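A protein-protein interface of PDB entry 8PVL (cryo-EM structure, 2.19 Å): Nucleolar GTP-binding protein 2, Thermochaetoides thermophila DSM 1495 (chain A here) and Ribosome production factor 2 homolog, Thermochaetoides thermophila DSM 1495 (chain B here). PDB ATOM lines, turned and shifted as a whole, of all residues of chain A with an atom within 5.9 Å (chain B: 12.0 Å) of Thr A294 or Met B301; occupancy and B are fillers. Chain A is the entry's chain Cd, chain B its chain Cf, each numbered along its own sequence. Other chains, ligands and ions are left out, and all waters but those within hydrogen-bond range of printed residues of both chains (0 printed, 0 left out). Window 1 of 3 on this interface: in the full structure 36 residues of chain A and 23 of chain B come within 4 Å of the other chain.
N of Phe A268 lies within hydrogen-bond range of O of Pro A293 (2.9 Å). N of Cys A295 lies within hydrogen-bond range of O of Phe A268 (2.9 Å). The backbone NH of Leu A270 lies within hydrogen-bond range of the backbone carbonyl oxygen of Cys A295. The backbone carbonyl oxygen (O) of His A292 sits at hydrogen-bond distance from the side-chain hydroxyl (OG1) of Thr A294 (2.9 Å). O of Asn B286 lies within hydrogen-bond range of N of Arg B298 (2.9 Å). NE2 of His B300 lies within hydrogen-bond range of OD1 of Asn B286 (2.8 Å).
Thr A294 touches just one residue of chain B: Met B301 (3.4 Å). Of chain A, only Tyr A103 (3.5 Å), Pro A293 (3.7 Å), Thr A294 (3.4 Å), Cys A295 (3.6 Å) and Leu A313 (3.7 Å) come within 4 Å of Met B301. No residue of chain B comes within 4 Å of Val A267. No residue of chain B comes within 4 Å of Phe A268. No residue of chain B comes within 4 Å of Ile A285. Leu A288 touches none of the printed residues of chain B. No residue of chain B comes within 4 Å of Gln A289. Pro A293 touches just these residues of chain B: Ile B299 (3.7 Å) and Met B301 (3.7 Å). Of chain B, only Met B301 (3.6 Å) comes within 4 Å of Cys A295. Printed residues of chain A within 4 Å of Arg B298: Tyr A103 (3.7 Å). Printed residues of chain B within 4 Å of Gln A316: Ile B299 and His B300. Printed residues of chain A within 4 Å of His B300: Gln A316. Asp B305 touches none of the printed residues of chain A. The nearest residue of chain B that does not touch Thr A294 is Thr B304 (6.8 Å). The nearest residue of chain A that does not touch Met B301 is Ser A309 (4.2 Å).
Of the 11 printed residues of chain B, 4 touch a printed residue of chain A. Hydrophobic or aromatic side chains of chain B within 4 Å of the printed part of chain A: Ile B299, His B300 and Met B301. Along chain B the printed residues that touch a printed residue of chain A span positions 298 to 301. Of the 17 printed residues of chain A, 6 touch a printed residue of chain B. Hydrophobic or aromatic side chains of chain A within 4 Å of the printed part of chain B: Tyr A103, Pro A293 and Leu A313. Among the printed residues, 10 pairs touch across the chains. Among the printed residues, no Asp or Glu carboxylate lies within 4 Å of a Lys or Arg side-chain nitrogen of the other chain.
The backbone NH (N) of Ile B299 lies within hydrogen-bond range of the backbone carbonyl oxygen (O) of Tyr A103 (3.2 Å). OE1 of Gln A316 sits at hydrogen-bond distance from N of His B300, at 2.8 Å.
Among the printed residues, merely in contact across the chains: Tyr A103 with Arg B298 (3.7 Å), Tyr A103 with Met B301 (3.5 Å), Pro A293 with Ile B299 (3.7 Å), Pro A293 with Met B301 (3.7 Å), Thr A294 with Met B301 (3.4 Å), Cys A295 with Met B301 (3.6 Å), Leu A313 with Met B301 (3.7 Å) and Gln A316 with Ile B299 (3.5 Å).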
ATOM      1  N   TYR A 103      -3.596  28.072 -10.478  1.00  0.00           N
ATOM      2  CA  TYR A 103      -2.634  27.134  -9.920  1.00  0.00           C
ATOM      3  C   TYR A 103      -2.538  27.233  -8.403  1.00  0.00           C
ATOM      4  O   TYR A 103      -1.568  26.746  -7.814  1.00  0.00           O
ATOM      5  CB  TYR A 103      -1.266  27.344 -10.564  1.00  0.00           C
ATOM      6  CG  TYR A 103      -1.309  27.156 -12.058  1.00  0.00           C
ATOM      7  CD1 TYR A 103      -1.407  25.889 -12.615  1.00  0.00           C
ATOM      8  CD2 TYR A 103      -1.256  28.247 -12.915  1.00  0.00           C
ATOM      9  CE1 TYR A 103      -1.457  25.716 -13.982  1.00  0.00           C
ATOM     10  CE2 TYR A 103      -1.300  28.082 -14.283  1.00  0.00           C
ATOM     11  CZ  TYR A 103      -1.401  26.814 -14.811  1.00  0.00           C
ATOM     12  OH  TYR A 103      -1.445  26.642 -16.175  1.00  0.00           O
ATOM     13  N   VAL A 267     -10.345  19.969 -11.412  1.00  0.00           N
ATOM     14  CA  VAL A 267      -9.277  19.748 -12.382  1.00  0.00           C
ATOM     15  C   VAL A 267      -9.887  19.216 -13.672  1.00  0.00           C
ATOM     16  O   VAL A 267     -10.587  18.200 -13.656  1.00  0.00           O
ATOM     17  CB  VAL A 267      -8.214  18.765 -11.849  1.00  0.00           C
ATOM     18  CG1 VAL A 267      -7.209  18.414 -12.934  1.00  0.00           C
ATOM     19  CG2 VAL A 267      -7.502  19.339 -10.637  1.00  0.00           C
ATOM     20  N   PHE A 268      -9.611  19.892 -14.786  1.00  0.00           N
ATOM     21  CA  PHE A 268     -10.009  19.397 -16.096  1.00  0.00           C
ATOM     22  C   PHE A 268      -9.083  18.277 -16.549  1.00  0.00           C
ATOM     23  O   PHE A 268      -7.863  18.345 -16.370  1.00  0.00           O
ATOM     24  CB  PHE A 268      -9.981  20.520 -17.132  1.00  0.00           C
ATOM     25  CG  PHE A 268     -11.158  21.438 -17.069  1.00  0.00           C
ATOM     26  CD1 PHE A 268     -12.444  20.933 -16.989  1.00  0.00           C
ATOM     27  CD2 PHE A 268     -10.980  22.810 -17.103  1.00  0.00           C
ATOM     28  CE1 PHE A 268     -13.530  21.782 -16.938  1.00  0.00           C
ATOM     29  CE2 PHE A 268     -12.062  23.662 -17.050  1.00  0.00           C
ATOM     30  CZ  PHE A 268     -13.338  23.148 -16.968  1.00  0.00           C
ATOM     31  N   VAL A 269      -9.665  17.244 -17.149  1.00  0.00           N
ATOM     32  CA  VAL A 269      -8.905  16.174 -17.783  1.00  0.00           C
ATOM     33  C   VAL A 269      -9.433  16.028 -19.202  1.00  0.00           C
ATOM     34  O   VAL A 269     -10.577  15.605 -19.404  1.00  0.00           O
ATOM     35  CB  VAL A 269      -9.007  14.845 -17.024  1.00  0.00           C
ATOM     36  CG1 VAL A 269      -8.330  13.745 -17.813  1.00  0.00           C
ATOM     37  CG2 VAL A 269      -8.378  14.963 -15.651  1.00  0.00           C
ATOM     38  N   LEU A 270      -8.603  16.367 -20.181  1.00  0.00           N
ATOM     39  CA  LEU A 270      -8.947  16.230 -21.590  1.00  0.00           C
ATOM     40  C   LEU A 270      -8.588  14.817 -22.031  1.00  0.00           C
ATOM     41  O   LEU A 270      -7.409  14.502 -22.225  1.00  0.00           O
ATOM     42  CB  LEU A 270      -8.208  17.275 -22.421  1.00  0.00           C
ATOM     43  CG  LEU A 270      -8.821  17.685 -23.758  1.00  0.00           C
ATOM     44  CD1 LEU A 270     -10.167  18.345 -23.547  1.00  0.00           C
ATOM     45  CD2 LEU A 270      -7.879  18.612 -24.503  1.00  0.00           C
ATOM     46  N   TRP A 284      -6.465  23.655 -27.074  1.00  0.00           N
ATOM     47  CA  TRP A 284      -7.563  23.505 -26.128  1.00  0.00           C
ATOM     48  C   TRP A 284      -7.066  23.485 -24.688  1.00  0.00           C
ATOM     49  O   TRP A 284      -7.756  23.984 -23.792  1.00  0.00           O
ATOM     50  CB  TRP A 284      -8.355  22.236 -26.442  1.00  0.00           C
ATOM     51  CG  TRP A 284      -9.409  22.420 -27.495  1.00  0.00           C
ATOM     52  CD1 TRP A 284      -9.456  21.819 -28.719  1.00  0.00           C
ATOM     53  CD2 TRP A 284     -10.572  23.253 -27.415  1.00  0.00           C
ATOM     54  NE1 TRP A 284     -10.572  22.225 -29.404  1.00  0.00           N
ATOM     55  CE2 TRP A 284     -11.275  23.106 -28.625  1.00  0.00           C
ATOM     56  CE3 TRP A 284     -11.090  24.105 -26.435  1.00  0.00           C
ATOM     57  CZ2 TRP A 284     -12.463  23.782 -28.884  1.00  0.00           C
ATOM     58  CZ3 TRP A 284     -12.267  24.775 -26.694  1.00  0.00           C
ATOM     59  CH2 TRP A 284     -12.941  24.610 -27.908  1.00  0.00           C
ATOM     60  N   ILE A 285      -5.879  22.920 -24.448  1.00  0.00           N
ATOM     61  CA  ILE A 285      -5.285  22.948 -23.114  1.00  0.00           C
ATOM     62  C   ILE A 285      -4.988  24.381 -22.691  1.00  0.00           C
ATOM     63  O   ILE A 285      -5.262  24.776 -21.549  1.00  0.00           O
ATOM     64  CB  ILE A 285      -4.018  22.070 -23.081  1.00  0.00           C
ATOM     65  CG1 ILE A 285      -4.393  20.597 -22.957  1.00  0.00           C
ATOM     66  CG2 ILE A 285      -3.095  22.456 -21.932  1.00  0.00           C
ATOM     67  CD1 ILE A 285      -3.213  19.689 -23.095  1.00  0.00           C
ATOM     68  N   LEU A 288      -8.319  25.970 -21.750  1.00  0.00           N
ATOM     69  CA  LEU A 288      -8.945  25.493 -20.517  1.00  0.00           C
ATOM     70  C   LEU A 288      -8.135  25.829 -19.268  1.00  0.00           C
ATOM     71  O   LEU A 288      -8.708  25.943 -18.171  1.00  0.00           O
ATOM     72  CB  LEU A 288      -9.173  23.982 -20.599  1.00  0.00           C
ATOM     73  CG  LEU A 288     -10.207  23.516 -21.626  1.00  0.00           C
ATOM     74  CD1 LEU A 288     -10.138  22.012 -21.814  1.00  0.00           C
ATOM     75  CD2 LEU A 288     -11.607  23.946 -21.227  1.00  0.00           C
ATOM     76  N   GLN A 289      -6.817  25.993 -19.402  1.00  0.00           N
ATOM     77  CA  GLN A 289      -5.991  26.291 -18.240  1.00  0.00           C
ATOM     78  C   GLN A 289      -6.143  27.723 -17.750  1.00  0.00           C
ATOM     79  O   GLN A 289      -5.630  28.047 -16.675  1.00  0.00           O
ATOM     80  CB  GLN A 289      -4.522  25.990 -18.539  1.00  0.00           C
ATOM     81  CG  GLN A 289      -3.846  26.973 -19.467  1.00  0.00           C
ATOM     82  CD  GLN A 289      -2.479  26.494 -19.903  1.00  0.00           C
ATOM     83  OE1 GLN A 289      -2.079  25.370 -19.601  1.00  0.00           O
ATOM     84  NE2 GLN A 289      -1.752  27.345 -20.615  1.00  0.00           N
ATOM     85  N   HIS A 292      -9.139  26.329 -15.219  1.00  0.00           N
ATOM     86  CA  HIS A 292      -8.806  25.294 -14.253  1.00  0.00           C
ATOM     87  C   HIS A 292      -7.588  24.523 -14.735  1.00  0.00           C
ATOM     88  O   HIS A 292      -7.321  24.477 -15.941  1.00  0.00           O
ATOM     89  CB  HIS A 292      -9.997  24.349 -14.035  1.00  0.00           C
ATOM     90  CG  HIS A 292     -11.124  24.971 -13.272  1.00  0.00           C
ATOM     91  ND1 HIS A 292     -12.217  25.539 -13.892  1.00  0.00           N
ATOM     92  CD2 HIS A 292     -11.321  25.132 -11.944  1.00  0.00           C
ATOM     93  CE1 HIS A 292     -13.041  26.015 -12.977  1.00  0.00           C
ATOM     94  NE2 HIS A 292     -12.521  25.781 -11.787  1.00  0.00           N
ATOM     95  N   PRO A 293      -6.816  23.928 -13.819  1.00  0.00           N
ATOM     96  CA  PRO A 293      -5.673  23.105 -14.243  1.00  0.00           C
ATOM     97  C   PRO A 293      -6.126  21.916 -15.075  1.00  0.00           C
ATOM     98  O   PRO A 293      -7.067  21.210 -14.716  1.00  0.00           O
ATOM     99  CB  PRO A 293      -5.046  22.652 -12.919  1.00  0.00           C
ATOM    100  CG  PRO A 293      -5.538  23.601 -11.909  1.00  0.00           C
ATOM    101  CD  PRO A 293      -6.884  24.052 -12.351  1.00  0.00           C
ATOM    102  N   THR A 294      -5.434  21.692 -16.190  1.00  0.00           N
ATOM    103  CA  THR A 294      -5.878  20.745 -17.204  1.00  0.00           C
ATOM    104  C   THR A 294      -4.788  19.720 -17.476  1.00  0.00           C
ATOM    105  O   THR A 294      -3.622  20.080 -17.657  1.00  0.00           O
ATOM    106  CB  THR A 294      -6.254  21.472 -18.501  1.00  0.00           C
ATOM    107  OG1 THR A 294      -7.075  22.605 -18.194  1.00  0.00           O
ATOM    108  CG2 THR A 294      -7.014  20.546 -19.435  1.00  0.00           C
ATOM    109  N   CYS A 295      -5.175  18.448 -17.505  1.00  0.00           N
ATOM    110  CA  CYS A 295      -4.280  17.346 -17.831  1.00  0.00           C
ATOM    111  C   CYS A 295      -4.725  16.680 -19.126  1.00  0.00           C
ATOM    112  O   CYS A 295      -5.895  16.328 -19.277  1.00  0.00           O
ATOM    113  CB  CYS A 295      -4.259  16.295 -16.715  1.00  0.00           C
ATOM    114  SG  CYS A 295      -3.761  16.880 -15.088  1.00  0.00           S
ATOM    115  N   ALA A 296      -3.789  16.490 -20.050  1.00  0.00           N
ATOM    116  CA  ALA A 296      -4.053  15.721 -21.259  1.00  0.00           C
ATOM    117  C   ALA A 296      -3.899  14.239 -20.961  1.00  0.00           C
ATOM    118  O   ALA A 296      -2.977  13.834 -20.247  1.00  0.00           O
ATOM    119  CB  ALA A 296      -3.104  16.124 -22.386  1.00  0.00           C
ATOM    120  N   SER A 309       1.828  12.203 -15.195  1.00  0.00           N
ATOM    121  CA  SER A 309       1.521  13.585 -14.842  1.00  0.00           C
ATOM    122  C   SER A 309       0.285  13.679 -13.953  1.00  0.00           C
ATOM    123  O   SER A 309       0.277  14.433 -12.967  1.00  0.00           O
ATOM    124  CB  SER A 309       1.335  14.412 -16.112  1.00  0.00           C
ATOM    125  OG  SER A 309       0.740  15.663 -15.821  1.00  0.00           O
ATOM    126  N   LEU A 313       0.061  15.018 -10.047  1.00  0.00           N
ATOM    127  CA  LEU A 313      -0.869  16.033  -9.554  1.00  0.00           C
ATOM    128  C   LEU A 313      -1.675  15.524  -8.361  1.00  0.00           C
ATOM    129  O   LEU A 313      -1.875  16.251  -7.373  1.00  0.00           O
ATOM    130  CB  LEU A 313      -1.800  16.485 -10.678  1.00  0.00           C
ATOM    131  CG  LEU A 313      -2.694  17.674 -10.330  1.00  0.00           C
ATOM    132  CD1 LEU A 313      -1.850  18.879  -9.956  1.00  0.00           C
ATOM    133  CD2 LEU A 313      -3.626  18.006 -11.478  1.00  0.00           C
ATOM    134  N   GLN A 316       0.519  15.590  -5.341  1.00  0.00           N
ATOM    135  CA  GLN A 316       0.618  16.941  -4.797  1.00  0.00           C
ATOM    136  C   GLN A 316      -0.603  17.287  -3.956  1.00  0.00           C
ATOM    137  O   GLN A 316      -0.472  17.872  -2.874  1.00  0.00           O
ATOM    138  CB  GLN A 316       0.789  17.956  -5.925  1.00  0.00           C
ATOM    139  CG  GLN A 316       2.116  17.868  -6.640  1.00  0.00           C
ATOM    140  CD  GLN A 316       2.248  18.887  -7.746  1.00  0.00           C
ATOM    141  OE1 GLN A 316       1.928  20.061  -7.565  1.00  0.00           O
ATOM    142  NE2 GLN A 316       2.713  18.443  -8.905  1.00  0.00           N
ATOM    143  N   ASN B 286       4.794  24.913  -0.311  1.00  0.00           N
ATOM    144  CA  ASN B 286       3.604  25.154  -1.130  1.00  0.00           C
ATOM    145  C   ASN B 286       2.394  25.629  -0.332  1.00  0.00           C
ATOM    146  O   ASN B 286       1.312  25.774  -0.907  1.00  0.00           O
ATOM    147  CB  ASN B 286       3.209  23.922  -1.955  1.00  0.00           C
ATOM    148  CG  ASN B 286       4.242  23.567  -3.001  1.00  0.00           C
ATOM    149  OD1 ASN B 286       4.715  24.429  -3.738  1.00  0.00           O
ATOM    150  ND2 ASN B 286       4.601  22.293  -3.068  1.00  0.00           N
ATOM    151  N   GLY B 297      -2.803  26.581  -1.059  1.00  0.00           N
ATOM    152  CA  GLY B 297      -1.830  25.602  -1.518  1.00  0.00           C
ATOM    153  C   GLY B 297      -1.519  25.808  -2.990  1.00  0.00           C
ATOM    154  O   GLY B 297      -2.410  26.114  -3.785  1.00  0.00           O
ATOM    155  N   ARG B 298      -0.250  25.638  -3.340  1.00  0.00           N
ATOM    156  CA  ARG B 298       0.231  25.828  -4.702  1.00  0.00           C
ATOM    157  C   ARG B 298       0.499  24.475  -5.346  1.00  0.00           C
ATOM    158  O   ARG B 298       1.131  23.607  -4.736  1.00  0.00           O
ATOM    159  CB  ARG B 298       1.498  26.686  -4.717  1.00  0.00           C
ATOM    160  CG  ARG B 298       2.073  26.919  -6.102  1.00  0.00           C
ATOM    161  CD  ARG B 298       2.856  28.214  -6.175  1.00  0.00           C
ATOM    162  NE  ARG B 298       1.979  29.376  -6.240  1.00  0.00           N
ATOM    163  CZ  ARG B 298       1.517  29.903  -7.366  1.00  0.00           C
ATOM    164  NH1 ARG B 298       1.818  29.384  -8.544  1.00  0.00           N
ATOM    165  NH2 ARG B 298       0.733  30.974  -7.308  1.00  0.00           N
ATOM    166  N   ILE B 299       0.014  24.300  -6.573  1.00  0.00           N
ATOM    167  CA  ILE B 299       0.228  23.080  -7.335  1.00  0.00           C
ATOM    168  C   ILE B 299       1.065  23.409  -8.565  1.00  0.00           C
ATOM    169  O   ILE B 299       1.119  24.551  -9.026  1.00  0.00           O
ATOM    170  CB  ILE B 299      -1.097  22.404  -7.741  1.00  0.00           C
ATOM    171  CG1 ILE B 299      -1.955  23.362  -8.563  1.00  0.00           C
ATOM    172  CG2 ILE B 299      -1.852  21.935  -6.511  1.00  0.00           C
ATOM    173  CD1 ILE B 299      -3.182  22.718  -9.143  1.00  0.00           C
ATOM    174  N   HIS B 300       1.726  22.382  -9.095  1.00  0.00           N
ATOM    175  CA  HIS B 300       2.671  22.534 -10.198  1.00  0.00           C
ATOM    176  C   HIS B 300       2.354  21.496 -11.265  1.00  0.00           C
ATOM    177  O   HIS B 300       2.593  20.302 -11.067  1.00  0.00           O
ATOM    178  CB  HIS B 300       4.107  22.394  -9.698  1.00  0.00           C
ATOM    179  CG  HIS B 300       4.411  23.255  -8.514  1.00  0.00           C
ATOM    180  ND1 HIS B 300       4.560  24.622  -8.607  1.00  0.00           N
ATOM    181  CD2 HIS B 300       4.559  22.951  -7.204  1.00  0.00           C
ATOM    182  CE1 HIS B 300       4.806  25.119  -7.409  1.00  0.00           C
ATOM    183  NE2 HIS B 300       4.811  24.126  -6.540  1.00  0.00           N
ATOM    184  N   MET B 301       1.819  21.958 -12.396  1.00  0.00           N
ATOM    185  CA  MET B 301       1.378  21.057 -13.455  1.00  0.00           C
ATOM    186  C   MET B 301       2.546  20.475 -14.242  1.00  0.00           C
ATOM    187  O   MET B 301       2.550  19.279 -14.556  1.00  0.00           O
ATOM    188  CB  MET B 301       0.428  21.795 -14.396  1.00  0.00           C
ATOM    189  CG  MET B 301      -0.847  22.257 -13.725  1.00  0.00           C
ATOM    190  SD  MET B 301      -1.796  20.894 -13.046  1.00  0.00           S
ATOM    191  CE  MET B 301      -2.333  20.124 -14.564  1.00  0.00           C
ATOM    192  N   GLY B 302       3.536  21.296 -14.573  1.00  0.00           N
ATOM    193  CA  GLY B 302       4.611  20.882 -15.448  1.00  0.00           C
ATOM    194  C   GLY B 302       4.337  21.227 -16.901  1.00  0.00           C
ATOM    195  O   GLY B 302       3.227  21.591 -17.297  1.00  0.00           O
ATOM    196  N   LYS B 303       5.384  21.111 -17.711  1.00  0.00           N
ATOM    197  CA  LYS B 303       5.299  21.467 -19.121  1.00  0.00           C
ATOM    198  C   LYS B 303       4.577  20.376 -19.902  1.00  0.00           C
ATOM    199  O   LYS B 303       4.880  19.189 -19.755  1.00  0.00           O
ATOM    200  CB  LYS B 303       6.695  21.696 -19.697  1.00  0.00           C
ATOM    201  N   THR B 304       3.624  20.784 -20.738  1.00  0.00           N
ATOM    202  CA  THR B 304       2.878  19.846 -21.567  1.00  0.00           C
ATOM    203  C   THR B 304       3.720  19.458 -22.777  1.00  0.00           C
ATOM    204  O   THR B 304       4.109  20.321 -23.572  1.00  0.00           O
ATOM    205  CB  THR B 304       1.551  20.459 -22.009  1.00  0.00           C
ATOM    206  N   ASP B 305       3.998  18.162 -22.918  1.00  0.00           N
ATOM    207  CA  ASP B 305       4.851  17.638 -23.986  1.00  0.00           C
ATOM    208  C   ASP B 305       4.069  16.567 -24.739  1.00  0.00           C
ATOM    209  O   ASP B 305       4.132  15.383 -24.399  1.00  0.00           O
ATOM    210  CB  ASP B 305       6.159  17.091 -23.422  1.00  0.00           C
ATOM    211  N   LEU B 306       3.340  16.989 -25.768  1.00  0.00           N
ATOM    212  CA  LEU B 306       2.536  16.094 -26.587  1.00  0.00           C
ATOM    213  C   LEU B 306       3.307  15.530 -27.772  1.00  0.00           C
ATOM    214  O   LEU B 306       2.710  14.861 -28.620  1.00  0.00           O
ATOM    215  CB  LEU B 306       1.285  16.820 -27.085  1.00  0.00           C
ATOM    216  CG  LEU B 306      -0.029  16.643 -26.320  1.00  0.00           C
ATOM    217  CD1 LEU B 306       0.136  16.885 -24.828  1.00  0.00           C
ATOM    218  CD2 LEU B 306      -1.080  17.572 -26.891  1.00  0.00           C
